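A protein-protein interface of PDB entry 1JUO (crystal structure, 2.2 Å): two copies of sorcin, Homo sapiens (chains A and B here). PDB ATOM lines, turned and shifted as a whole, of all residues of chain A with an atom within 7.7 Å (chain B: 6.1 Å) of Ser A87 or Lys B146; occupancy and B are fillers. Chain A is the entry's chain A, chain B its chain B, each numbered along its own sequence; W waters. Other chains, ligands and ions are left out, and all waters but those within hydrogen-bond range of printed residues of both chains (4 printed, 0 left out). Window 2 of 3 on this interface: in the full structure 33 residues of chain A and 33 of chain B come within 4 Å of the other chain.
The backbone carbonyl oxygen of Ser A197 is in hydrogen-bond range of the side-chain hydroxyl of Ser A80 (2.7 Å). N of Met A86 is in hydrogen-bond range of OD2 of Asp A83, 3.1 Å away. The backbone NH of Ser A87 sits at hydrogen-bond distance from the side-chain carboxylate of Asp A83, at 2.9 Å. OG of Ser A87 lies within hydrogen-bond range of OG1 of Thr A89, at 2.5 Å.
Among the printed residues, pairs that only touch across the chains: Arg A76 with Arg B147, Met A86 with Ser B143, Met A86 with Lys B146, Ser A87 with Lys B146, Met A196 with Ile B144, Met A196 with Arg B147, Ser A197 with Ser B143 and Ser A197 with Arg B147.
Ser A87 touches one residue of chain B. Ala B145 touches none of the printed residues of chain A. Of the printed residues of chain B, Arg A76 touches Arg B147 (3.98 Å). Printed residues of chain A within 4 Å of Ser B143: Met A86 (3.8 Å) and Ser A197 (3.3 Å). Ile A49 touches none of the printed residues of chain B. Ala A51 touches none of the printed residues of chain B. The nearest printed residue of chain A that does not touch Ile B144 is Ser A197 (5.3 Å).
Hydrophobic or aromatic side chains of chain B that line the printed part of chain A: Ile B144. Along chain B the printed residues that touch a printed residue of chain A span positions 143 to 147. Of the 19 printed residues of chain A, 5 touch a printed residue of chain B. Hydrophobic or aromatic side chains of chain A that line the printed part of chain B: Met A86 and Met A196.
No position is printed for both chains. Of the 8 pairs that touch across the chains among the printed residues, none has its exchanged pair printed and touching as well.
Water W3 bridges O of Met A196 (2.7 Å) and OH of Tyr B148 (3.1 Å). Water W1 lies within hydrogen-bond range of O of Met A196 (2.8 Å) and NE of Arg B147 (3.0 Å). Water W2 lies within hydrogen-bond range of the side-chain amide oxygen of Asn B142 (2.8 Å) and the backbone carbonyl oxygen of Met A86 (2.8 Å). Water W4 bridges the guanidinium group of Arg A76 (3.1 Å) and the backbone carbonyl oxygen of Ser B149 (3.4 Å).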
ATOM      1  N   GLN A  48      18.403 -19.094 -23.221  1.00  0.00           N
ATOM      2  CA  GLN A  48      18.855 -18.914 -21.847  1.00  0.00           C
ATOM      3  C   GLN A  48      18.068 -19.832 -20.900  1.00  0.00           C
ATOM      4  O   GLN A  48      16.890 -20.077 -21.118  1.00  0.00           O
ATOM      5  CB  GLN A  48      18.674 -17.444 -21.459  1.00  0.00           C
ATOM      6  CG  GLN A  48      19.788 -16.886 -20.610  1.00  0.00           C
ATOM      7  CD  GLN A  48      21.099 -16.765 -21.348  1.00  0.00           C
ATOM      8  OE1 GLN A  48      22.157 -16.886 -20.747  1.00  0.00           O
ATOM      9  NE2 GLN A  48      21.041 -16.510 -22.651  1.00  0.00           N
ATOM     10  N   ILE A  49      18.716 -20.353 -19.862  1.00  0.00           N
ATOM     11  CA  ILE A  49      18.035 -21.252 -18.917  1.00  0.00           C
ATOM     12  C   ILE A  49      18.269 -20.886 -17.450  1.00  0.00           C
ATOM     13  O   ILE A  49      19.380 -20.504 -17.073  1.00  0.00           O
ATOM     14  CB  ILE A  49      18.498 -22.720 -19.088  1.00  0.00           C
ATOM     15  CG1 ILE A  49      20.007 -22.822 -18.835  1.00  0.00           C
ATOM     16  CG2 ILE A  49      18.151 -23.220 -20.473  1.00  0.00           C
ATOM     17  CD1 ILE A  49      20.572 -24.246 -18.875  1.00  0.00           C
ATOM     18  N   ASP A  50      17.233 -21.004 -16.623  1.00  0.00           N
ATOM     19  CA  ASP A  50      17.389 -20.714 -15.200  1.00  0.00           C
ATOM     20  C   ASP A  50      17.770 -22.004 -14.475  1.00  0.00           C
ATOM     21  O   ASP A  50      17.900 -23.053 -15.110  1.00  0.00           O
ATOM     22  CB  ASP A  50      16.109 -20.128 -14.599  1.00  0.00           C
ATOM     23  CG  ASP A  50      14.914 -21.036 -14.760  1.00  0.00           C
ATOM     24  OD1 ASP A  50      15.085 -22.274 -14.712  1.00  0.00           O
ATOM     25  OD2 ASP A  50      13.792 -20.505 -14.914  1.00  0.00           O
ATOM     26  N   ALA A  51      17.944 -21.927 -13.156  1.00  0.00           N
ATOM     27  CA  ALA A  51      18.347 -23.083 -12.352  1.00  0.00           C
ATOM     28  C   ALA A  51      17.380 -24.238 -12.466  1.00  0.00           C
ATOM     29  O   ALA A  51      17.782 -25.402 -12.425  1.00  0.00           O
ATOM     30  CB  ALA A  51      18.493 -22.684 -10.892  1.00  0.00           C
ATOM     31  N   ARG A  76      21.233 -24.094  -8.611  1.00  0.00           N
ATOM     32  CA  ARG A  76      21.259 -22.664  -8.370  1.00  0.00           C
ATOM     33  C   ARG A  76      22.695 -22.223  -8.218  1.00  0.00           C
ATOM     34  O   ARG A  76      23.079 -21.155  -8.697  1.00  0.00           O
ATOM     35  CB  ARG A  76      20.465 -22.326  -7.110  1.00  0.00           C
ATOM     36  CG  ARG A  76      18.987 -22.134  -7.379  1.00  0.00           C
ATOM     37  CD  ARG A  76      18.194 -21.891  -6.111  1.00  0.00           C
ATOM     38  NE  ARG A  76      16.860 -21.390  -6.424  1.00  0.00           N
ATOM     39  CZ  ARG A  76      15.930 -21.121  -5.516  1.00  0.00           C
ATOM     40  NH1 ARG A  76      16.183 -21.314  -4.231  1.00  0.00           N
ATOM     41  NH2 ARG A  76      14.757 -20.631  -5.890  1.00  0.00           N
ATOM     42  N   VAL A  79      24.335 -22.183 -11.713  1.00  0.00           N
ATOM     43  CA  VAL A  79      24.023 -21.007 -12.500  1.00  0.00           C
ATOM     44  C   VAL A  79      24.908 -19.870 -11.985  1.00  0.00           C
ATOM     45  O   VAL A  79      25.593 -19.197 -12.748  1.00  0.00           O
ATOM     46  CB  VAL A  79      22.523 -20.609 -12.357  1.00  0.00           C
ATOM     47  CG1 VAL A  79      22.247 -19.309 -13.109  1.00  0.00           C
ATOM     48  CG2 VAL A  79      21.637 -21.716 -12.900  1.00  0.00           C
ATOM     49  N   SER A  80      24.905 -19.681 -10.674  1.00  0.00           N
ATOM     50  CA  SER A  80      25.689 -18.620 -10.060  1.00  0.00           C
ATOM     51  C   SER A  80      27.171 -18.699 -10.428  1.00  0.00           C
ATOM     52  O   SER A  80      27.814 -17.684 -10.699  1.00  0.00           O
ATOM     53  CB  SER A  80      25.520 -18.681  -8.543  1.00  0.00           C
ATOM     54  OG  SER A  80      26.158 -17.591  -7.915  1.00  0.00           O
ATOM     55  N   ASP A  83      27.398 -17.393 -14.053  1.00  0.00           N
ATOM     56  CA  ASP A  83      26.593 -16.219 -14.373  1.00  0.00           C
ATOM     57  C   ASP A  83      27.414 -14.924 -14.522  1.00  0.00           C
ATOM     58  O   ASP A  83      27.241 -13.973 -13.757  1.00  0.00           O
ATOM     59  CB  ASP A  83      25.533 -16.053 -13.282  1.00  0.00           C
ATOM     60  CG  ASP A  83      24.460 -15.069 -13.665  1.00  0.00           C
ATOM     61  OD1 ASP A  83      23.594 -14.774 -12.815  1.00  0.00           O
ATOM     62  OD2 ASP A  83      24.489 -14.593 -14.818  1.00  0.00           O
ATOM     63  N   ARG A  84      28.280 -14.879 -15.529  1.00  0.00           N
ATOM     64  CA  ARG A  84      29.137 -13.720 -15.749  1.00  0.00           C
ATOM     65  C   ARG A  84      28.450 -12.359 -15.871  1.00  0.00           C
ATOM     66  O   ARG A  84      29.055 -11.338 -15.544  1.00  0.00           O
ATOM     67  CB  ARG A  84      30.031 -13.960 -16.969  1.00  0.00           C
ATOM     68  CG  ARG A  84      30.945 -15.161 -16.809  1.00  0.00           C
ATOM     69  CD  ARG A  84      31.983 -15.279 -17.926  1.00  0.00           C
ATOM     70  NE  ARG A  84      32.885 -16.412 -17.703  1.00  0.00           N
ATOM     71  CZ  ARG A  84      32.590 -17.688 -17.953  1.00  0.00           C
ATOM     72  NH1 ARG A  84      31.410 -18.023 -18.450  1.00  0.00           N
ATOM     73  NH2 ARG A  84      33.476 -18.638 -17.685  1.00  0.00           N
ATOM     74  N   ASP A  85      27.202 -12.318 -16.321  1.00  0.00           N
ATOM     75  CA  ASP A  85      26.519 -11.030 -16.456  1.00  0.00           C
ATOM     76  C   ASP A  85      25.379 -10.853 -15.463  1.00  0.00           C
ATOM     77  O   ASP A  85      24.515  -9.999 -15.646  1.00  0.00           O
ATOM     78  CB  ASP A  85      25.980 -10.860 -17.874  1.00  0.00           C
ATOM     79  CG  ASP A  85      25.016 -11.949 -18.254  1.00  0.00           C
ATOM     80  OD1 ASP A  85      24.420 -11.864 -19.346  1.00  0.00           O
ATOM     81  OD2 ASP A  85      24.858 -12.899 -17.457  1.00  0.00           O
ATOM     82  N   MET A  86      25.383 -11.672 -14.415  1.00  0.00           N
ATOM     83  CA  MET A  86      24.363 -11.619 -13.375  1.00  0.00           C
ATOM     84  C   MET A  86      22.911 -11.548 -13.840  1.00  0.00           C
ATOM     85  O   MET A  86      22.152 -10.685 -13.393  1.00  0.00           O
ATOM     86  CB  MET A  86      24.654 -10.454 -12.431  1.00  0.00           C
ATOM     87  CG  MET A  86      25.789 -10.748 -11.461  1.00  0.00           C
ATOM     88  SD  MET A  86      25.565 -12.357 -10.606  1.00  0.00           S
ATOM     89  CE  MET A  86      24.233 -11.974  -9.427  1.00  0.00           C
ATOM     90  N   SER A  87      22.512 -12.470 -14.711  1.00  0.00           N
ATOM     91  CA  SER A  87      21.138 -12.481 -15.200  1.00  0.00           C
ATOM     92  C   SER A  87      20.329 -13.610 -14.573  1.00  0.00           C
ATOM     93  O   SER A  87      19.129 -13.741 -14.818  1.00  0.00           O
ATOM     94  CB  SER A  87      21.121 -12.632 -16.716  1.00  0.00           C
ATOM     95  OG  SER A  87      21.505 -13.936 -17.092  1.00  0.00           O
ATOM     96  N   GLY A  88      20.993 -14.427 -13.765  1.00  0.00           N
ATOM     97  CA  GLY A  88      20.319 -15.538 -13.125  1.00  0.00           C
ATOM     98  C   GLY A  88      20.024 -16.639 -14.122  1.00  0.00           C
ATOM     99  O   GLY A  88      19.267 -17.568 -13.837  1.00  0.00           O
ATOM    100  N   THR A  89      20.629 -16.537 -15.301  1.00  0.00           N
ATOM    101  CA  THR A  89      20.416 -17.530 -16.344  1.00  0.00           C
ATOM    102  C   THR A  89      21.733 -17.982 -16.935  1.00  0.00           C
ATOM    103  O   THR A  89      22.791 -17.492 -16.559  1.00  0.00           O
ATOM    104  CB  THR A  89      19.535 -16.979 -17.467  1.00  0.00           C
ATOM    105  OG1 THR A  89      20.178 -15.845 -18.060  1.00  0.00           O
ATOM    106  CG2 THR A  89      18.188 -16.558 -16.921  1.00  0.00           C
ATOM    107  N   MET A  90      21.662 -18.912 -17.877  1.00  0.00           N
ATOM    108  CA  MET A  90      22.862 -19.455 -18.490  1.00  0.00           C
ATOM    109  C   MET A  90      22.638 -19.749 -19.964  1.00  0.00           C
ATOM    110  O   MET A  90      21.573 -20.239 -20.347  1.00  0.00           O
ATOM    111  CB  MET A  90      23.242 -20.736 -17.750  1.00  0.00           C
ATOM    112  CG  MET A  90      24.427 -21.484 -18.283  1.00  0.00           C
ATOM    113  SD  MET A  90      24.594 -23.043 -17.369  1.00  0.00           S
ATOM    114  CE  MET A  90      24.887 -22.444 -15.719  1.00  0.00           C
ATOM    115  N   GLY A  91      23.645 -19.438 -20.781  1.00  0.00           N
ATOM    116  CA  GLY A  91      23.576 -19.683 -22.212  1.00  0.00           C
ATOM    117  C   GLY A  91      24.214 -21.013 -22.577  1.00  0.00           C
ATOM    118  O   GLY A  91      24.886 -21.636 -21.756  1.00  0.00           O
ATOM    119  N   GLU A  94      27.920 -21.498 -21.900  1.00  0.00           N
ATOM    120  CA  GLU A  94      28.172 -21.659 -20.476  1.00  0.00           C
ATOM    121  C   GLU A  94      27.820 -23.084 -20.065  1.00  0.00           C
ATOM    122  O   GLU A  94      28.514 -23.686 -19.247  1.00  0.00           O
ATOM    123  CB  GLU A  94      27.356 -20.654 -19.656  1.00  0.00           C
ATOM    124  CG  GLU A  94      27.747 -19.202 -19.885  1.00  0.00           C
ATOM    125  CD  GLU A  94      26.911 -18.536 -20.959  1.00  0.00           C
ATOM    126  OE1 GLU A  94      25.810 -18.035 -20.636  1.00  0.00           O
ATOM    127  OE2 GLU A  94      27.347 -18.523 -22.129  1.00  0.00           O
ATOM    128  N   MET A 196      26.708 -14.025  -0.990  1.00  0.00           N
ATOM    129  CA  MET A 196      25.270 -14.264  -1.083  1.00  0.00           C
ATOM    130  C   MET A 196      24.885 -14.804  -2.459  1.00  0.00           C
ATOM    131  O   MET A 196      23.821 -15.391  -2.618  1.00  0.00           O
ATOM    132  CB  MET A 196      24.478 -12.985  -0.795  1.00  0.00           C
ATOM    133  CG  MET A 196      24.432 -12.593   0.678  1.00  0.00           C
ATOM    134  SD  MET A 196      23.678 -13.856   1.735  1.00  0.00           S
ATOM    135  CE  MET A 196      21.948 -13.528   1.472  1.00  0.00           C
ATOM    136  N   SER A 197      25.738 -14.610  -3.462  1.00  0.00           N
ATOM    137  CA  SER A 197      25.428 -15.128  -4.798  1.00  0.00           C
ATOM    138  C   SER A 197      25.672 -16.623  -4.814  1.00  0.00           C
ATOM    139  O   SER A 197      24.975 -17.367  -5.503  1.00  0.00           O
ATOM    140  CB  SER A 197      26.322 -14.487  -5.867  1.00  0.00           C
ATOM    141  OG  SER A 197      26.200 -13.059  -5.842  1.00  0.00           O
ATOM    142  N   VAL B 141      22.034  -6.165  -3.134  1.00  0.00           N
ATOM    143  CA  VAL B 141      20.626  -6.532  -3.183  1.00  0.00           C
ATOM    144  C   VAL B 141      20.304  -7.231  -4.493  1.00  0.00           C
ATOM    145  O   VAL B 141      19.487  -8.146  -4.535  1.00  0.00           O
ATOM    146  CB  VAL B 141      19.719  -5.299  -3.062  1.00  0.00           C
ATOM    147  CG1 VAL B 141      18.266  -5.720  -3.108  1.00  0.00           C
ATOM    148  CG2 VAL B 141      20.011  -4.577  -1.775  1.00  0.00           C
ATOM    149  N   ASN B 142      20.956  -6.800  -5.566  1.00  0.00           N
ATOM    150  CA  ASN B 142      20.719  -7.385  -6.875  1.00  0.00           C
ATOM    151  C   ASN B 142      21.324  -8.785  -6.966  1.00  0.00           C
ATOM    152  O   ASN B 142      20.798  -9.653  -7.661  1.00  0.00           O
ATOM    153  CB  ASN B 142      21.288  -6.473  -7.952  1.00  0.00           C
ATOM    154  CG  ASN B 142      20.461  -6.493  -9.215  1.00  0.00           C
ATOM    155  OD1 ASN B 142      20.626  -7.368 -10.069  1.00  0.00           O
ATOM    156  ND2 ASN B 142      19.540  -5.537  -9.333  1.00  0.00           N
ATOM    157  N   SER B 143      22.428  -9.004  -6.255  1.00  0.00           N
ATOM    158  CA  SER B 143      23.072 -10.311  -6.234  1.00  0.00           C
ATOM    159  C   SER B 143      22.131 -11.271  -5.533  1.00  0.00           C
ATOM    160  O   SER B 143      21.895 -12.380  -6.004  1.00  0.00           O
ATOM    161  CB  SER B 143      24.398 -10.264  -5.469  1.00  0.00           C
ATOM    162  OG  SER B 143      25.408  -9.596  -6.204  1.00  0.00           O
ATOM    163  N   ILE B 144      21.594 -10.828  -4.400  1.00  0.00           N
ATOM    164  CA  ILE B 144      20.666 -11.632  -3.606  1.00  0.00           C
ATOM    165  C   ILE B 144      19.432 -12.020  -4.415  1.00  0.00           C
ATOM    166  O   ILE B 144      19.080 -13.196  -4.517  1.00  0.00           O
ATOM    167  CB  ILE B 144      20.207 -10.859  -2.353  1.00  0.00           C
ATOM    168  CG1 ILE B 144      21.407 -10.584  -1.448  1.00  0.00           C
ATOM    169  CG2 ILE B 144      19.134 -11.643  -1.614  1.00  0.00           C
ATOM    170  CD1 ILE B 144      21.085  -9.688  -0.265  1.00  0.00           C
ATOM    171  N   ALA B 145      18.780 -11.018  -4.994  1.00  0.00           N
ATOM    172  CA  ALA B 145      17.580 -11.248  -5.786  1.00  0.00           C
ATOM    173  C   ALA B 145      17.775 -12.238  -6.936  1.00  0.00           C
ATOM    174  O   ALA B 145      16.982 -13.158  -7.092  1.00  0.00           O
ATOM    175  CB  ALA B 145      17.060  -9.924  -6.320  1.00  0.00           C
ATOM    176  N   LYS B 146      18.824 -12.052  -7.732  1.00  0.00           N
ATOM    177  CA  LYS B 146      19.086 -12.925  -8.869  1.00  0.00           C
ATOM    178  C   LYS B 146      19.313 -14.386  -8.502  1.00  0.00           C
ATOM    179  O   LYS B 146      18.956 -15.283  -9.268  1.00  0.00           O
ATOM    180  CB  LYS B 146      20.287 -12.407  -9.671  1.00  0.00           C
ATOM    181  CG  LYS B 146      20.003 -11.152 -10.483  1.00  0.00           C
ATOM    182  CD  LYS B 146      18.972 -11.423 -11.571  1.00  0.00           C
ATOM    183  CE  LYS B 146      18.751 -10.206 -12.456  1.00  0.00           C
ATOM    184  NZ  LYS B 146      17.809 -10.515 -13.571  1.00  0.00           N
ATOM    185  N   ARG B 147      19.896 -14.623  -7.332  1.00  0.00           N
ATOM    186  CA  ARG B 147      20.200 -15.975  -6.888  1.00  0.00           C
ATOM    187  C   ARG B 147      18.975 -16.642  -6.324  1.00  0.00           C
ATOM    188  O   ARG B 147      18.798 -17.873  -6.451  1.00  0.00           O
ATOM    189  CB  ARG B 147      21.300 -15.942  -5.827  1.00  0.00           C
ATOM    190  CG  ARG B 147      21.038 -16.785  -4.611  1.00  0.00           C
ATOM    191  CD  ARG B 147      21.631 -18.153  -4.812  1.00  0.00           C
ATOM    192  NE  ARG B 147      21.128 -19.108  -3.839  1.00  0.00           N
ATOM    193  CZ  ARG B 147      21.672 -20.295  -3.622  1.00  0.00           C
ATOM    194  NH1 ARG B 147      22.742 -20.704  -4.284  1.00  0.00           N
ATOM    195  NH2 ARG B 147      21.109 -21.107  -2.728  1.00  0.00           N
ATOM    196  N   TYR B 148      18.147 -15.829  -5.676  1.00  0.00           N
ATOM    197  CA  TYR B 148      16.917 -16.295  -5.044  1.00  0.00           C
ATOM    198  C   TYR B 148      15.670 -15.999  -5.838  1.00  0.00           C
ATOM    199  O   TYR B 148      14.587 -15.976  -5.268  1.00  0.00           O
ATOM    200  CB  TYR B 148      16.747 -15.664  -3.672  1.00  0.00           C
ATOM    201  CG  TYR B 148      17.641 -16.289  -2.679  1.00  0.00           C
ATOM    202  CD1 TYR B 148      18.560 -15.528  -1.987  1.00  0.00           C
ATOM    203  CD2 TYR B 148      17.540 -17.648  -2.407  1.00  0.00           C
ATOM    204  CE1 TYR B 148      19.367 -16.100  -1.025  1.00  0.00           C
ATOM    205  CE2 TYR B 148      18.337 -18.225  -1.458  1.00  0.00           C
ATOM    206  CZ  TYR B 148      19.258 -17.441  -0.766  1.00  0.00           C
ATOM    207  OH  TYR B 148      20.087 -18.040   0.146  1.00  0.00           O
ATOM    208  N   SER B 149      15.810 -15.771  -7.135  1.00  0.00           N
ATOM    209  CA  SER B 149      14.646 -15.438  -7.949  1.00  0.00           C
ATOM    210  C   SER B 149      13.952 -16.547  -8.752  1.00  0.00           C
ATOM    211  O   SER B 149      14.298 -16.791  -9.925  1.00  0.00           O
ATOM    212  CB  SER B 149      14.996 -14.265  -8.898  1.00  0.00           C
ATOM    213  OG  SER B 149      14.880 -14.600 -10.274  1.00  0.00           O
HETATM  214  O   HOH W   1      23.277 -18.072  -1.959  1.00  0.00           O
HETATM  215  O   HOH W   2      21.648  -8.005 -12.617  1.00  0.00           O
HETATM  216  O   HOH W   3      22.170 -15.827  -0.520  1.00  0.00           O
HETATM  217  O   HOH W   4      15.928 -19.564  -8.688  1.00  0.00           O
